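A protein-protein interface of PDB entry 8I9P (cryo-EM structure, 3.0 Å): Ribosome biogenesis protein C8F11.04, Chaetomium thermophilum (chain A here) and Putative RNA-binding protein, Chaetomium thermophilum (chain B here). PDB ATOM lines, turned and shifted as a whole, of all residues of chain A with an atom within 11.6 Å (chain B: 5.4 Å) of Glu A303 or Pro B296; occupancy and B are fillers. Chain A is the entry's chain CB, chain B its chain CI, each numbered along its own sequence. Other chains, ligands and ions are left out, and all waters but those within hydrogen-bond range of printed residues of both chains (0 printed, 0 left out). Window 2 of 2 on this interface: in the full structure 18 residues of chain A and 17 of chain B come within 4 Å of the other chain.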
ATOM      1  N   LYS A  69      27.740  19.638  27.051  1.00  0.00           N
ATOM      2  CA  LYS A  69      26.977  19.516  25.778  1.00  0.00           C
ATOM      3  C   LYS A  69      27.882  19.855  24.588  1.00  0.00           C
ATOM      4  O   LYS A  69      27.789  19.151  23.565  1.00  0.00           O
ATOM      5  CB  LYS A  69      25.750  20.432  25.816  1.00  0.00           C
ATOM      6  CG  LYS A  69      24.758  20.133  26.932  1.00  0.00           C
ATOM      7  CD  LYS A  69      23.677  21.179  27.075  1.00  0.00           C
ATOM      8  CE  LYS A  69      22.800  20.955  28.288  1.00  0.00           C
ATOM      9  NZ  LYS A  69      21.754  21.999  28.407  1.00  0.00           N
ATOM     10  N   LYS A  70      28.720  20.888  24.722  1.00  0.00           N
ATOM     11  CA  LYS A  70      29.629  21.306  23.620  1.00  0.00           C
ATOM     12  C   LYS A  70      31.089  21.091  24.033  1.00  0.00           C
ATOM     13  O   LYS A  70      31.321  20.452  25.078  1.00  0.00           O
ATOM     14  CB  LYS A  70      29.385  22.777  23.275  1.00  0.00           C
ATOM     15  CG  LYS A  70      29.397  23.725  24.466  1.00  0.00           C
ATOM     16  CD  LYS A  70      29.374  25.187  24.081  1.00  0.00           C
ATOM     17  CE  LYS A  70      30.646  25.635  23.394  1.00  0.00           C
ATOM     18  NZ  LYS A  70      30.633  27.090  23.112  1.00  0.00           N
ATOM     19  N   HIS A  71      32.034  21.601  23.238  1.00  0.00           N
ATOM     20  CA  HIS A  71      33.443  21.484  23.580  1.00  0.00           C
ATOM     21  C   HIS A  71      33.850  22.543  24.598  1.00  0.00           C
ATOM     22  O   HIS A  71      33.560  23.731  24.432  1.00  0.00           O
ATOM     23  CB  HIS A  71      34.291  21.609  22.320  1.00  0.00           C
ATOM     24  CG  HIS A  71      34.364  20.345  21.523  1.00  0.00           C
ATOM     25  ND1 HIS A  71      35.348  20.106  20.590  1.00  0.00           N
ATOM     26  CD2 HIS A  71      33.565  19.252  21.514  1.00  0.00           C
ATOM     27  CE1 HIS A  71      35.158  18.918  20.047  1.00  0.00           C
ATOM     28  NE2 HIS A  71      34.080  18.379  20.589  1.00  0.00           N
ATOM     29  N   GLN A 273      30.188  29.278  29.584  1.00  0.00           N
ATOM     30  CA  GLN A 273      28.777  29.633  29.826  1.00  0.00           C
ATOM     31  C   GLN A 273      28.181  28.878  31.025  1.00  0.00           C
ATOM     32  O   GLN A 273      27.013  28.483  31.039  1.00  0.00           O
ATOM     33  CB  GLN A 273      27.929  29.504  28.542  1.00  0.00           C
ATOM     34  CG  GLN A 273      27.583  28.127  27.972  1.00  0.00           C
ATOM     35  CD  GLN A 273      26.743  28.219  26.712  1.00  0.00           C
ATOM     36  OE1 GLN A 273      26.636  29.283  26.099  1.00  0.00           O
ATOM     37  NE2 GLN A 273      26.137  27.104  26.320  1.00  0.00           N
ATOM     38  N   GLN A 276      25.005  25.666  32.914  1.00  0.00           N
ATOM     39  CA  GLN A 276      24.049  25.101  31.979  1.00  0.00           C
ATOM     40  C   GLN A 276      24.638  23.972  31.164  1.00  0.00           C
ATOM     41  O   GLN A 276      23.974  22.952  30.961  1.00  0.00           O
ATOM     42  CB  GLN A 276      23.515  26.241  31.092  1.00  0.00           C
ATOM     43  CG  GLN A 276      22.399  26.011  30.046  1.00  0.00           C
ATOM     44  CD  GLN A 276      22.766  25.334  28.717  1.00  0.00           C
ATOM     45  OE1 GLN A 276      23.613  24.450  28.573  1.00  0.00           O
ATOM     46  NE2 GLN A 276      22.094  25.792  27.694  1.00  0.00           N
ATOM     47  N   ASN A 277      25.848  24.180  30.627  1.00  0.00           N
ATOM     48  CA  ASN A 277      26.492  23.172  29.735  1.00  0.00           C
ATOM     49  C   ASN A 277      26.562  21.804  30.412  1.00  0.00           C
ATOM     50  O   ASN A 277      26.517  20.792  29.689  1.00  0.00           O
ATOM     51  CB  ASN A 277      27.901  23.599  29.317  1.00  0.00           C
ATOM     52  CG  ASN A 277      27.936  24.374  28.019  1.00  0.00           C
ATOM     53  OD1 ASN A 277      26.939  24.448  27.304  1.00  0.00           O
ATOM     54  ND2 ASN A 277      29.086  24.944  27.701  1.00  0.00           N
ATOM     55  N   GLU A 298      17.044  19.793  30.441  1.00  0.00           N
ATOM     56  CA  GLU A 298      17.060  20.381  29.110  1.00  0.00           C
ATOM     57  C   GLU A 298      18.435  20.159  28.491  1.00  0.00           C
ATOM     58  O   GLU A 298      19.452  20.182  29.189  1.00  0.00           O
ATOM     59  CB  GLU A 298      16.707  21.875  29.204  1.00  0.00           C
ATOM     60  CG  GLU A 298      16.941  22.711  27.965  1.00  0.00           C
ATOM     61  CD  GLU A 298      17.102  24.180  28.296  1.00  0.00           C
ATOM     62  OE1 GLU A 298      16.381  24.668  29.190  1.00  0.00           O
ATOM     63  OE2 GLU A 298      17.943  24.850  27.663  1.00  0.00           O
ATOM     64  N   LEU A 299      18.463  19.930  27.171  1.00  0.00           N
ATOM     65  CA  LEU A 299      19.687  19.564  26.463  1.00  0.00           C
ATOM     66  C   LEU A 299      20.058  20.563  25.366  1.00  0.00           C
ATOM     67  O   LEU A 299      20.805  20.227  24.446  1.00  0.00           O
ATOM     68  CB  LEU A 299      19.570  18.160  25.867  1.00  0.00           C
ATOM     69  CG  LEU A 299      19.289  16.950  26.765  1.00  0.00           C
ATOM     70  CD1 LEU A 299      17.797  16.678  26.901  1.00  0.00           C
ATOM     71  CD2 LEU A 299      20.005  15.720  26.227  1.00  0.00           C
ATOM     72  N   TRP A 300      19.568  21.800  25.454  1.00  0.00           N
ATOM     73  CA  TRP A 300      19.877  22.823  24.457  1.00  0.00           C
ATOM     74  C   TRP A 300      20.162  24.149  25.151  1.00  0.00           C
ATOM     75  O   TRP A 300      20.361  24.166  26.368  1.00  0.00           O
ATOM     76  CB  TRP A 300      18.732  22.954  23.451  1.00  0.00           C
ATOM     77  CG  TRP A 300      17.388  23.138  24.084  1.00  0.00           C
ATOM     78  CD1 TRP A 300      16.860  24.299  24.566  1.00  0.00           C
ATOM     79  CD2 TRP A 300      16.400  22.123  24.310  1.00  0.00           C
ATOM     80  NE1 TRP A 300      15.604  24.073  25.075  1.00  0.00           N
ATOM     81  CE2 TRP A 300      15.297  22.746  24.927  1.00  0.00           C
ATOM     82  CE3 TRP A 300      16.340  20.751  24.047  1.00  0.00           C
ATOM     83  CZ2 TRP A 300      14.150  22.044  25.291  1.00  0.00           C
ATOM     84  CZ3 TRP A 300      15.199  20.055  24.407  1.00  0.00           C
ATOM     85  CH2 TRP A 300      14.120  20.704  25.022  1.00  0.00           C
ATOM     86  N   LEU A 301      20.225  25.265  24.412  1.00  0.00           N
ATOM     87  CA  LEU A 301      20.464  26.553  25.061  1.00  0.00           C
ATOM     88  C   LEU A 301      19.292  27.512  24.892  1.00  0.00           C
ATOM     89  O   LEU A 301      18.616  27.814  25.878  1.00  0.00           O
ATOM     90  CB  LEU A 301      21.781  27.132  24.526  1.00  0.00           C
ATOM     91  CG  LEU A 301      22.410  28.497  24.870  1.00  0.00           C
ATOM     92  CD1 LEU A 301      22.791  28.654  26.346  1.00  0.00           C
ATOM     93  CD2 LEU A 301      23.578  28.859  23.944  1.00  0.00           C
ATOM     94  N   ASP A 302      19.027  28.002  23.687  1.00  0.00           N
ATOM     95  CA  ASP A 302      17.759  28.630  23.349  1.00  0.00           C
ATOM     96  C   ASP A 302      17.452  28.246  21.914  1.00  0.00           C
ATOM     97  O   ASP A 302      16.297  28.227  21.478  1.00  0.00           O
ATOM     98  CB  ASP A 302      17.822  30.148  23.525  1.00  0.00           C
ATOM     99  CG  ASP A 302      16.515  30.830  23.175  1.00  0.00           C
ATOM    100  OD1 ASP A 302      15.448  30.227  23.412  1.00  0.00           O
ATOM    101  OD2 ASP A 302      16.552  31.971  22.668  1.00  0.00           O
ATOM    102  N   GLU A 303      18.517  27.923  21.183  1.00  0.00           N
ATOM    103  CA  GLU A 303      18.442  27.571  19.769  1.00  0.00           C
ATOM    104  C   GLU A 303      18.090  26.091  19.674  1.00  0.00           C
ATOM    105  O   GLU A 303      18.648  25.230  20.359  1.00  0.00           O
ATOM    106  CB  GLU A 303      19.737  27.992  19.057  1.00  0.00           C
ATOM    107  CG  GLU A 303      21.122  27.410  19.489  1.00  0.00           C
ATOM    108  CD  GLU A 303      21.366  25.922  19.270  1.00  0.00           C
ATOM    109  OE1 GLU A 303      20.672  25.289  18.451  1.00  0.00           O
ATOM    110  OE2 GLU A 303      22.349  25.409  19.842  1.00  0.00           O
ATOM    111  N   SER A 304      17.073  25.819  18.865  1.00  0.00           N
ATOM    112  CA  SER A 304      16.544  24.484  18.641  1.00  0.00           C
ATOM    113  C   SER A 304      15.616  24.544  17.441  1.00  0.00           C
ATOM    114  O   SER A 304      14.599  25.238  17.467  1.00  0.00           O
ATOM    115  CB  SER A 304      15.796  23.958  19.870  1.00  0.00           C
ATOM    116  OG  SER A 304      14.688  24.782  20.187  1.00  0.00           O
ATOM    117  N   GLU B 294      27.667  22.079  18.043  1.00  0.00           N
ATOM    118  CA  GLU B 294      27.122  23.434  18.110  1.00  0.00           C
ATOM    119  C   GLU B 294      25.909  23.591  17.199  1.00  0.00           C
ATOM    120  O   GLU B 294      24.998  24.370  17.500  1.00  0.00           O
ATOM    121  CB  GLU B 294      28.211  24.452  17.749  1.00  0.00           C
ATOM    122  CG  GLU B 294      27.912  25.916  18.116  1.00  0.00           C
ATOM    123  CD  GLU B 294      27.038  26.640  17.102  1.00  0.00           C
ATOM    124  OE1 GLU B 294      27.067  26.258  15.914  1.00  0.00           O
ATOM    125  OE2 GLU B 294      26.324  27.589  17.492  1.00  0.00           O
ATOM    126  N   ARG B 295      25.885  22.857  16.080  1.00  0.00           N
ATOM    127  CA  ARG B 295      24.947  23.031  14.974  1.00  0.00           C
ATOM    128  C   ARG B 295      23.495  22.845  15.407  1.00  0.00           C
ATOM    129  O   ARG B 295      23.171  21.875  16.102  1.00  0.00           O
ATOM    130  CB  ARG B 295      25.295  22.059  13.845  1.00  0.00           C
ATOM    131  CG  ARG B 295      24.365  22.136  12.644  1.00  0.00           C
ATOM    132  CD  ARG B 295      24.781  21.200  11.483  1.00  0.00           C
ATOM    133  NE  ARG B 295      26.189  21.093  11.074  1.00  0.00           N
ATOM    134  CZ  ARG B 295      27.103  22.059  10.965  1.00  0.00           C
ATOM    135  NH1 ARG B 295      26.799  23.342  11.093  1.00  0.00           N
ATOM    136  NH2 ARG B 295      28.356  21.726  10.674  1.00  0.00           N
ATOM    137  N   PRO B 296      22.599  23.760  15.027  1.00  0.00           N
ATOM    138  CA  PRO B 296      21.212  23.701  15.513  1.00  0.00           C
ATOM    139  C   PRO B 296      20.393  22.643  14.785  1.00  0.00           C
ATOM    140  O   PRO B 296      20.202  22.716  13.569  1.00  0.00           O
ATOM    141  CB  PRO B 296      20.678  25.112  15.228  1.00  0.00           C
ATOM    142  CG  PRO B 296      21.898  25.955  14.986  1.00  0.00           C
ATOM    143  CD  PRO B 296      22.867  25.028  14.331  1.00  0.00           C
ATOM    144  N   LEU B 297      19.913  21.658  15.538  1.00  0.00           N
ATOM    145  CA  LEU B 297      18.834  20.802  15.066  1.00  0.00           C
ATOM    146  C   LEU B 297      17.491  21.501  15.279  1.00  0.00           C
ATOM    147  O   LEU B 297      17.307  22.261  16.234  1.00  0.00           O
ATOM    148  CB  LEU B 297      18.860  19.443  15.776  1.00  0.00           C
ATOM    149  CG  LEU B 297      20.035  18.464  15.620  1.00  0.00           C
ATOM    150  CD1 LEU B 297      20.427  18.298  14.151  1.00  0.00           C
ATOM    151  CD2 LEU B 297      21.242  18.802  16.488  1.00  0.00           C
ATOM    152  N   SER B 298      16.539  21.246  14.376  1.00  0.00           N
ATOM    153  CA  SER B 298      15.386  22.140  14.312  1.00  0.00           C
ATOM    154  C   SER B 298      14.185  21.754  15.178  1.00  0.00           C
ATOM    155  O   SER B 298      13.891  22.458  16.147  1.00  0.00           O
ATOM    156  CB  SER B 298      14.935  22.277  12.856  1.00  0.00           C
ATOM    157  OG  SER B 298      15.972  22.807  12.048  1.00  0.00           O
ATOM    158  N   TRP B 302      15.532  16.778  17.880  1.00  0.00           N
ATOM    159  CA  TRP B 302      15.603  16.812  19.341  1.00  0.00           C
ATOM    160  C   TRP B 302      14.685  15.763  19.964  1.00  0.00           C
ATOM    161  O   TRP B 302      14.941  15.284  21.076  1.00  0.00           O
ATOM    162  CB  TRP B 302      15.268  18.203  19.881  1.00  0.00           C
ATOM    163  CG  TRP B 302      16.252  19.254  19.485  1.00  0.00           C
ATOM    164  CD1 TRP B 302      16.197  20.057  18.385  1.00  0.00           C
ATOM    165  CD2 TRP B 302      17.476  19.580  20.158  1.00  0.00           C
ATOM    166  NE1 TRP B 302      17.290  20.887  18.350  1.00  0.00           N
ATOM    167  CE2 TRP B 302      18.095  20.609  19.422  1.00  0.00           C
ATOM    168  CE3 TRP B 302      18.101  19.110  21.316  1.00  0.00           C
ATOM    169  CZ2 TRP B 302      19.307  21.176  19.807  1.00  0.00           C
ATOM    170  CZ3 TRP B 302      19.305  19.672  21.696  1.00  0.00           C
ATOM    171  CH2 TRP B 302      19.896  20.694  20.942  1.00  0.00           C
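The backbone carbonyl oxygen (O) of Trp A300 lies within hydrogen-bond range of the side-chain amino group (NZ) of Lys A69, at 3.3 Å.
NE2 of Gln A276 lies within hydrogen-bond range of O of Trp A300 (2.7 Å).
O of Leu B297 sits at hydrogen-bond distance from NE1 of Trp B302 (2.5 Å).
O of Ser A304 sits close to O of Ser B298 (3.2 Å).
Printed residues of chain A that touch a printed residue of chain B: Leu A299, Trp A300, Glu A303 and Ser A304.
Hydrophobic or aromatic side chains of chain A that line the printed part of chain B: Trp A300.
Among the printed residues, 7 pairs touch across the chains.
Among the printed residues, no Asp or Glu carboxylate lies within 4 Å of a Lys or Arg side-chain nitrogen of the other chain.
Among the printed residues, merely in contact across the chains: Ser A304 with Leu B297, Leu A299 with Trp B302, Glu A303 with Pro B296, Trp A300 with Trp B302, Ser A304 with Trp B302 and Glu A303 with Glu B294.
Of chain B, only Glu B294 and Pro B296 come within 4 Å of Glu A303.
Of chain A, only Glu A303 (3.2 Å) comes within 4 Å of Pro B296.
Glu B294 touches one residue of chain A.
Of chain A, only Ser A304 comes within 4 Å of Leu B297.
Of the printed residues of chain B, Trp A300 touches Trp B302.
Of the printed residues of chain B, Ser A304 touches Leu B297, Ser B298 and Trp B302.
Of the printed residues of chain A, Trp B302 touches Leu A299 (3.2 Å), Trp A300 (3.6 Å) and Ser A304 (3.7 Å).
Of the printed residues of chain B, Leu A299 touches Trp B302.
The nearest residue of chain B that does not touch Glu A303 is Trp B302 (4.1 Å).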
